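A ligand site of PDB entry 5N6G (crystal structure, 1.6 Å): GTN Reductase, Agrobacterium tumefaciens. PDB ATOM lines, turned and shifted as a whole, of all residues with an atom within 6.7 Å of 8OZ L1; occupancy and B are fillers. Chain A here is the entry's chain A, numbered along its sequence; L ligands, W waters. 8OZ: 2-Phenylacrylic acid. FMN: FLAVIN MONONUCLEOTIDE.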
ATOM      1  N   PRO A  23      10.280 -17.189 -14.614  1.00  0.00           N
ATOM      2  CA  PRO A  23      11.279 -17.866 -15.451  1.00  0.00           C
ATOM      3  C   PRO A  23      10.663 -18.275 -16.789  1.00  0.00           C
ATOM      4  O   PRO A  23       9.562 -18.834 -16.838  1.00  0.00           O
ATOM      5  CB  PRO A  23      11.660 -19.089 -14.626  1.00  0.00           C
ATOM      6  CG  PRO A  23      10.462 -19.343 -13.720  1.00  0.00           C
ATOM      7  CD  PRO A  23       9.935 -17.962 -13.402  1.00  0.00           C
ATOM      8  N   LEU A  24      11.381 -17.992 -17.877  1.00  0.00           N
ATOM      9  CA  LEU A  24      10.864 -18.250 -19.214  1.00  0.00           C
ATOM     10  C   LEU A  24      11.951 -18.812 -20.121  1.00  0.00           C
ATOM     11  O   LEU A  24      12.775 -18.057 -20.649  1.00  0.00           O
ATOM     12  CB  LEU A  24      10.296 -16.977 -19.814  1.00  0.00           C
ATOM     13  CG  LEU A  24       9.125 -16.344 -19.062  1.00  0.00           C
ATOM     14  CD1 LEU A  24       9.056 -14.851 -19.389  1.00  0.00           C
ATOM     15  CD2 LEU A  24       7.849 -17.062 -19.443  1.00  0.00           C
ATOM     16  N   THR A  25      11.906 -20.125 -20.360  1.00  0.00           N
ATOM     17  CA  THR A  25      12.759 -20.776 -21.363  1.00  0.00           C
ATOM     18  C   THR A  25      12.461 -20.232 -22.754  1.00  0.00           C
ATOM     19  O   THR A  25      11.317 -20.225 -23.219  1.00  0.00           O
ATOM     20  CB  THR A  25      12.492 -22.288 -21.316  1.00  0.00           C
ATOM     21  OG1 THR A  25      12.968 -22.791 -20.062  1.00  0.00           O
ATOM     22  CG2 THR A  25      13.227 -23.032 -22.427  1.00  0.00           C
ATOM     23  N   ASN A  27      15.139 -20.774 -25.412  1.00  0.00           N
ATOM     24  CA  ASN A  27      15.981 -21.553 -26.335  1.00  0.00           C
ATOM     25  C   ASN A  27      16.750 -20.702 -27.341  1.00  0.00           C
ATOM     26  O   ASN A  27      16.785 -20.975 -28.548  1.00  0.00           O
ATOM     27  CB  ASN A  27      15.154 -22.593 -27.086  1.00  0.00           C
ATOM     28  CG  ASN A  27      14.268 -23.378 -26.166  1.00  0.00           C
ATOM     29  OD1 ASN A  27      13.099 -23.042 -25.993  1.00  0.00           O
ATOM     30  ND2 ASN A  27      14.805 -24.437 -25.571  1.00  0.00           N
ATOM     31  N   GLU A  54      15.255 -17.703 -17.137  1.00  0.00           N
ATOM     32  CA  GLU A  54      14.943 -18.999 -17.727  1.00  0.00           C
ATOM     33  C   GLU A  54      15.646 -20.104 -16.959  1.00  0.00           C
ATOM     34  O   GLU A  54      16.732 -19.909 -16.416  1.00  0.00           O
ATOM     35  CB  GLU A  54      15.401 -19.025 -19.187  1.00  0.00           C
ATOM     36  CG  GLU A  54      16.910 -18.917 -19.416  1.00  0.00           C
ATOM     37  CD  GLU A  54      17.267 -18.263 -20.750  1.00  0.00           C
ATOM     38  OE1 GLU A  54      17.262 -18.950 -21.802  1.00  0.00           O
ATOM     39  OE2 GLU A  54      17.537 -17.042 -20.749  1.00  0.00           O
ATOM     40  N   GLY A  55      15.059 -21.288 -16.950  1.00  0.00           N
ATOM     41  CA  GLY A  55      15.734 -22.405 -16.318  1.00  0.00           C
ATOM     42  C   GLY A  55      17.127 -22.562 -16.880  1.00  0.00           C
ATOM     43  O   GLY A  55      17.332 -22.496 -18.107  1.00  0.00           O
ATOM     44  N   TYR A  65      16.487 -29.600 -23.168  1.00  0.00           N
ATOM     45  CA  TYR A  65      16.113 -28.902 -24.402  1.00  0.00           C
ATOM     46  C   TYR A  65      17.359 -28.283 -25.007  1.00  0.00           C
ATOM     47  O   TYR A  65      18.295 -27.914 -24.297  1.00  0.00           O
ATOM     48  CB  TYR A  65      15.068 -27.794 -24.178  1.00  0.00           C
ATOM     49  CG  TYR A  65      13.876 -28.272 -23.380  1.00  0.00           C
ATOM     50  CD1 TYR A  65      13.935 -28.331 -22.016  1.00  0.00           C
ATOM     51  CD2 TYR A  65      12.736 -28.746 -24.012  1.00  0.00           C
ATOM     52  CE1 TYR A  65      12.888 -28.783 -21.281  1.00  0.00           C
ATOM     53  CE2 TYR A  65      11.681 -29.229 -23.270  1.00  0.00           C
ATOM     54  CZ  TYR A  65      11.753 -29.229 -21.902  1.00  0.00           C
ATOM     55  OH  TYR A  65      10.716 -29.711 -21.133  1.00  0.00           O
ATOM     56  N   GLN A  97      17.474 -19.440 -12.095  1.00  0.00           N
ATOM     57  CA  GLN A  97      16.626 -20.604 -11.840  1.00  0.00           C
ATOM     58  C   GLN A  97      17.436 -21.854 -12.150  1.00  0.00           C
ATOM     59  O   GLN A  97      17.499 -22.287 -13.292  1.00  0.00           O
ATOM     60  CB  GLN A  97      15.329 -20.585 -12.652  1.00  0.00           C
ATOM     61  CG  GLN A  97      14.430 -21.716 -12.165  1.00  0.00           C
ATOM     62  CD  GLN A  97      13.186 -21.980 -12.973  1.00  0.00           C
ATOM     63  OE1 GLN A  97      13.229 -22.181 -14.191  1.00  0.00           O
ATOM     64  NE2 GLN A  97      12.070 -22.049 -12.288  1.00  0.00           N
ATOM     65  N   TRP A  99      18.483 -25.621 -12.528  1.00  0.00           N
ATOM     66  CA  TRP A  99      17.549 -26.576 -13.107  1.00  0.00           C
ATOM     67  C   TRP A  99      18.213 -27.937 -13.302  1.00  0.00           C
ATOM     68  O   TRP A  99      19.375 -28.036 -13.673  1.00  0.00           O
ATOM     69  CB  TRP A  99      17.121 -26.040 -14.443  1.00  0.00           C
ATOM     70  CG  TRP A  99      15.947 -26.648 -15.123  1.00  0.00           C
ATOM     71  CD1 TRP A  99      14.966 -27.450 -14.597  1.00  0.00           C
ATOM     72  CD2 TRP A  99      15.584 -26.411 -16.485  1.00  0.00           C
ATOM     73  NE1 TRP A  99      14.018 -27.723 -15.560  1.00  0.00           N
ATOM     74  CE2 TRP A  99      14.379 -27.108 -16.728  1.00  0.00           C
ATOM     75  CE3 TRP A  99      16.173 -25.687 -17.519  1.00  0.00           C
ATOM     76  CZ2 TRP A  99      13.749 -27.082 -17.966  1.00  0.00           C
ATOM     77  CZ3 TRP A  99      15.570 -25.654 -18.740  1.00  0.00           C
ATOM     78  CH2 TRP A  99      14.370 -26.357 -18.971  1.00  0.00           C
ATOM     79  N   TYR A 129      13.138 -30.556 -27.571  1.00  0.00           N
ATOM     80  CA  TYR A 129      13.726 -29.885 -28.731  1.00  0.00           C
ATOM     81  C   TYR A 129      15.192 -30.277 -28.777  1.00  0.00           C
ATOM     82  O   TYR A 129      15.934 -30.038 -27.821  1.00  0.00           O
ATOM     83  CB  TYR A 129      13.568 -28.358 -28.630  1.00  0.00           C
ATOM     84  CG  TYR A 129      12.310 -27.877 -27.902  1.00  0.00           C
ATOM     85  CD1 TYR A 129      11.119 -28.582 -27.961  1.00  0.00           C
ATOM     86  CD2 TYR A 129      12.336 -26.690 -27.165  1.00  0.00           C
ATOM     87  CE1 TYR A 129       9.992 -28.142 -27.295  1.00  0.00           C
ATOM     88  CE2 TYR A 129      11.196 -26.241 -26.506  1.00  0.00           C
ATOM     89  CZ  TYR A 129      10.036 -26.976 -26.576  1.00  0.00           C
ATOM     90  OH  TYR A 129       8.897 -26.543 -25.925  1.00  0.00           O
ATOM     91  N   HIS A 178      14.629 -24.787  -9.150  1.00  0.00           N
ATOM     92  CA  HIS A 178      13.482 -25.275  -9.921  1.00  0.00           C
ATOM     93  C   HIS A 178      12.992 -26.583  -9.331  1.00  0.00           C
ATOM     94  O   HIS A 178      13.563 -27.649  -9.598  1.00  0.00           O
ATOM     95  CB  HIS A 178      13.856 -25.453 -11.380  1.00  0.00           C
ATOM     96  CG  HIS A 178      12.675 -25.515 -12.291  1.00  0.00           C
ATOM     97  ND1 HIS A 178      11.421 -25.897 -11.884  1.00  0.00           N
ATOM     98  CD2 HIS A 178      12.556 -25.205 -13.611  1.00  0.00           C
ATOM     99  CE1 HIS A 178      10.575 -25.816 -12.888  1.00  0.00           C
ATOM    100  NE2 HIS A 178      11.239 -25.409 -13.961  1.00  0.00           N
ATOM    101  N   ALA A 180       9.638 -27.517  -9.680  1.00  0.00           N
ATOM    102  CA  ALA A 180       8.312 -27.394 -10.228  1.00  0.00           C
ATOM    103  C   ALA A 180       8.225 -28.118 -11.581  1.00  0.00           C
ATOM    104  O   ALA A 180       9.197 -28.703 -12.067  1.00  0.00           O
ATOM    105  CB  ALA A 180       7.920 -25.909 -10.369  1.00  0.00           C
ATOM    106  N   ASN A 181       7.021 -28.120 -12.116  1.00  0.00           N
ATOM    107  CA  ASN A 181       6.700 -28.487 -13.509  1.00  0.00           C
ATOM    108  C   ASN A 181       7.266 -29.831 -13.946  1.00  0.00           C
ATOM    109  O   ASN A 181       7.628 -30.021 -15.102  1.00  0.00           O
ATOM    110  CB  ASN A 181       7.142 -27.383 -14.459  1.00  0.00           C
ATOM    111  CG  ASN A 181       6.447 -26.088 -14.155  1.00  0.00           C
ATOM    112  OD1 ASN A 181       5.323 -26.080 -13.650  1.00  0.00           O
ATOM    113  ND2 ASN A 181       7.094 -24.987 -14.449  1.00  0.00           N
ATOM    114  N   TYR A 183       9.918 -31.644 -13.271  1.00  0.00           N
ATOM    115  CA  TYR A 183      11.336 -31.901 -13.477  1.00  0.00           C
ATOM    116  C   TYR A 183      11.888 -32.727 -12.316  1.00  0.00           C
ATOM    117  O   TYR A 183      11.132 -33.374 -11.591  1.00  0.00           O
ATOM    118  CB  TYR A 183      12.058 -30.589 -13.765  1.00  0.00           C
ATOM    119  CG  TYR A 183      11.580 -30.041 -15.106  1.00  0.00           C
ATOM    120  CD1 TYR A 183      11.859 -30.697 -16.282  1.00  0.00           C
ATOM    121  CD2 TYR A 183      10.803 -28.887 -15.177  1.00  0.00           C
ATOM    122  CE1 TYR A 183      11.438 -30.211 -17.518  1.00  0.00           C
ATOM    123  CE2 TYR A 183      10.353 -28.411 -16.413  1.00  0.00           C
ATOM    124  CZ  TYR A 183      10.685 -29.068 -17.562  1.00  0.00           C
ATOM    125  OH  TYR A 183      10.256 -28.612 -18.791  1.00  0.00           O
ATOM    126  N   ARG A 230      10.930 -22.716  -6.412  1.00  0.00           N
ATOM    127  CA  ARG A 230       9.660 -22.684  -7.129  1.00  0.00           C
ATOM    128  C   ARG A 230       8.937 -24.016  -6.968  1.00  0.00           C
ATOM    129  O   ARG A 230       9.532 -25.077  -7.201  1.00  0.00           O
ATOM    130  CB  ARG A 230       9.860 -22.378  -8.612  1.00  0.00           C
ATOM    131  CG  ARG A 230       8.546 -22.058  -9.302  1.00  0.00           C
ATOM    132  CD  ARG A 230       8.711 -21.578 -10.713  1.00  0.00           C
ATOM    133  NE  ARG A 230       7.721 -20.553 -11.017  1.00  0.00           N
ATOM    134  CZ  ARG A 230       7.160 -20.337 -12.206  1.00  0.00           C
ATOM    135  NH1 ARG A 230       7.424 -21.118 -13.230  1.00  0.00           N
ATOM    136  NH2 ARG A 230       6.325 -19.332 -12.354  1.00  0.00           N
ATOM    137  N   ALA A 237       2.137 -30.662 -15.906  1.00  0.00           N
ATOM    138  CA  ALA A 237       3.265 -30.517 -16.814  1.00  0.00           C
ATOM    139  C   ALA A 237       4.124 -31.774 -16.845  1.00  0.00           C
ATOM    140  O   ALA A 237       4.435 -32.368 -15.813  1.00  0.00           O
ATOM    141  CB  ALA A 237       4.117 -29.323 -16.373  1.00  0.00           C
ATOM    142  N   ASN A 238       4.567 -32.137 -18.043  1.00  0.00           N
ATOM    143  CA  ASN A 238       5.535 -33.203 -18.237  1.00  0.00           C
ATOM    144  C   ASN A 238       5.065 -34.532 -17.641  1.00  0.00           C
ATOM    145  O   ASN A 238       5.846 -35.329 -17.119  1.00  0.00           O
ATOM    146  CB  ASN A 238       6.901 -32.768 -17.717  1.00  0.00           C
ATOM    147  CG  ASN A 238       7.469 -31.632 -18.567  1.00  0.00           C
ATOM    148  OD1 ASN A 238       7.527 -31.758 -19.791  1.00  0.00           O
ATOM    149  ND2 ASN A 238       7.757 -30.495 -17.938  1.00  0.00           N
ATOM    150  N   THR A 271       0.248 -25.066 -14.882  1.00  0.00           N
ATOM    151  CA  THR A 271       1.154 -24.054 -15.402  1.00  0.00           C
ATOM    152  C   THR A 271       0.690 -23.612 -16.775  1.00  0.00           C
ATOM    153  O   THR A 271       0.647 -24.419 -17.714  1.00  0.00           O
ATOM    154  CB  THR A 271       2.570 -24.608 -15.485  1.00  0.00           C
ATOM    155  OG1 THR A 271       2.878 -25.328 -14.282  1.00  0.00           O
ATOM    156  CG2 THR A 271       3.552 -23.448 -15.642  1.00  0.00           C
ATOM    157  N   TYR A 356       9.773 -19.914 -28.516  1.00  0.00           N
ATOM    158  CA  TYR A 356      10.882 -20.858 -28.389  1.00  0.00           C
ATOM    159  C   TYR A 356      11.749 -20.833 -29.631  1.00  0.00           C
ATOM    160  O   TYR A 356      11.260 -21.043 -30.739  1.00  0.00           O
ATOM    161  CB  TYR A 356      10.373 -22.277 -28.171  1.00  0.00           C
ATOM    162  CG  TYR A 356       9.356 -22.371 -27.062  1.00  0.00           C
ATOM    163  CD1 TYR A 356       9.750 -22.197 -25.750  1.00  0.00           C
ATOM    164  CD2 TYR A 356       8.027 -22.612 -27.331  1.00  0.00           C
ATOM    165  CE1 TYR A 356       8.839 -22.263 -24.726  1.00  0.00           C
ATOM    166  CE2 TYR A 356       7.110 -22.681 -26.314  1.00  0.00           C
ATOM    167  CZ  TYR A 356       7.514 -22.508 -25.024  1.00  0.00           C
ATOM    168  OH  TYR A 356       6.609 -22.571 -23.994  1.00  0.00           O
HETATM  169  C4  8OZ L   1       8.421 -24.316 -21.563  1.00  0.00           C
HETATM  170  C5  8OZ L   1       9.245 -24.931 -22.478  1.00  0.00           C
HETATM  171  C6  8OZ L   1      10.346 -25.636 -22.041  1.00  0.00           C
HETATM  172  C7  8OZ L   1      10.628 -25.714 -20.687  1.00  0.00           C
HETATM  173  C8  8OZ L   1       9.112 -25.313 -17.297  1.00  0.00           C
HETATM  174  C   8OZ L   1      11.441 -24.889 -17.945  1.00  0.00           C
HETATM  175  O   8OZ L   1       9.347 -25.163 -16.119  1.00  0.00           O
HETATM  176  C1  8OZ L   1      10.184 -25.073 -18.312  1.00  0.00           C
HETATM  177  C2  8OZ L   1       9.809 -25.080 -19.757  1.00  0.00           C
HETATM  178  C3  8OZ L   1       8.690 -24.394 -20.212  1.00  0.00           C
HETATM  179  O1  8OZ L   1       7.940 -25.706 -17.734  1.00  0.00           O
HETATM  180  N1  FMN L   2       8.490 -22.091 -15.797  1.00  0.00           N
HETATM  181  C2  FMN L   2       9.672 -22.373 -15.140  1.00  0.00           C
HETATM  182  O2  FMN L   2       9.687 -22.652 -13.927  1.00  0.00           O
HETATM  183  N3  FMN L   2      10.860 -22.310 -15.827  1.00  0.00           N
HETATM  184  C4  FMN L   2      11.010 -22.032 -17.174  1.00  0.00           C
HETATM  185  O4  FMN L   2      12.127 -21.954 -17.686  1.00  0.00           O
HETATM  186  C4A FMN L   2       9.762 -21.763 -17.866  1.00  0.00           C
HETATM  187  N5  FMN L   2       9.821 -21.462 -19.136  1.00  0.00           N
HETATM  188  C5A FMN L   2       8.638 -21.057 -19.752  1.00  0.00           C
HETATM  189  C6  FMN L   2       8.701 -20.610 -21.065  1.00  0.00           C
HETATM  190  C7  FMN L   2       7.575 -20.087 -21.685  1.00  0.00           C
HETATM  191  C7M FMN L   2       7.698 -19.589 -23.112  1.00  0.00           C
HETATM  192  C8  FMN L   2       6.364 -20.015 -21.001  1.00  0.00           C
HETATM  193  C8M FMN L   2       5.143 -19.384 -21.621  1.00  0.00           C
HETATM  194  C9  FMN L   2       6.286 -20.471 -19.685  1.00  0.00           C
HETATM  195  C9A FMN L   2       7.425 -20.979 -19.055  1.00  0.00           C
HETATM  196  N10 FMN L   2       7.410 -21.348 -17.694  1.00  0.00           N
HETATM  197  C10 FMN L   2       8.558 -21.775 -17.081  1.00  0.00           C
HETATM  198  C1' FMN L   2       6.197 -21.092 -16.914  1.00  0.00           C
HETATM  199  C2' FMN L   2       6.096 -19.617 -16.534  1.00  0.00           C
HETATM  200  O2' FMN L   2       7.152 -19.257 -15.630  1.00  0.00           O
HETATM  201  C3' FMN L   2       4.760 -19.255 -15.894  1.00  0.00           C
HETATM  202  O3' FMN L   2       4.529 -20.088 -14.760  1.00  0.00           O
HETATM  203  C4' FMN L   2       3.564 -19.391 -16.841  1.00  0.00           C
HETATM  204  O4' FMN L   2       3.824 -18.670 -18.056  1.00  0.00           O
HETATM  205  C5' FMN L   2       2.263 -18.932 -16.205  1.00  0.00           C
HETATM  206  O5' FMN L   2       2.335 -17.524 -15.867  1.00  0.00           O
HETATM  207  P   FMN L   2       1.615 -16.350 -16.722  1.00  0.00           P
HETATM  208  O1P FMN L   2       0.131 -16.644 -16.633  1.00  0.00           O
HETATM  209  O2P FMN L   2       2.126 -16.504 -18.139  1.00  0.00           O
HETATM  210  O3P FMN L   2       2.036 -15.092 -16.038  1.00  0.00           O
HETATM  211  O   HOH W   1       7.509 -27.745 -19.655  1.00  0.00           O
HETATM  212  O   HOH W   2       5.323 -25.813 -17.517  1.00  0.00           O
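O4 of FMN L2 sits at hydrogen-bond distance from N of Gly 55 (3.1 Å). O of Pro 23 is in hydrogen-bond range of O2' of FMN L2 (2.7 Å). O2 of FMN L2 sits at hydrogen-bond distance from NH1 of Arg 230. O4 of FMN L2 is in hydrogen-bond range of OG1 of Thr 25 (2.7 Å). ND2 of Asn 181 is in hydrogen-bond range of O of 8OZ L1 (2.8 Å). A ring nitrogen (NE2) of His 178 lies within hydrogen-bond range of an oxygen (O2) of FMN L2, at 3.2 Å. N of Thr 25 lies within hydrogen-bond range of N5 of FMN L2, at 2.8 Å. A ring nitrogen (NE2) of His 178 is in hydrogen-bond range of an oxygen (O) of 8OZ L1, 2.9 Å away. OE1 of Gln 97 is in hydrogen-bond range of N3 of FMN L2 (2.9 Å). A nitrogen (N1) of FMN L2 sits at hydrogen-bond distance from the side-chain amide nitrogen of Asn 181 (3.5 Å).
An oxygen (O) of 8OZ L1 sits close to a nitrogen (N3) of FMN L2, at 3.2 Å.
OG1 of Thr 271 lies within hydrogen-bond range of OD1 of Asn 181 (2.6 Å). ND2 of Asn 238 lies within hydrogen-bond range of OH of Tyr 183 (3.2 Å). The side-chain hydroxyl (OH) of Tyr 183 sits at hydrogen-bond distance from the side-chain hydroxyl (OH) of Tyr 65, at 2.6 Å. O of Asn 181 sits at hydrogen-bond distance from ND2 of Asn 238, 2.9 Å away. N of Ala 180 lies within hydrogen-bond range of ND1 of His 178 (3.3 Å).
Residues that only touch 8OZ L1: Trp 99 (3.2 Å), Thr 25 (3.3 Å), Tyr 183 (3.4 Å), Tyr 356 (3.5 Å), Tyr 129 (3.8 Å) and Tyr 65 (3.9 Å).
Water W1 lies within hydrogen-bond range of O1 of 8OZ L1 (2.8 Å), OH of Tyr 183 (3.0 Å) and ND2 of Asn 238 (3.3 Å).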
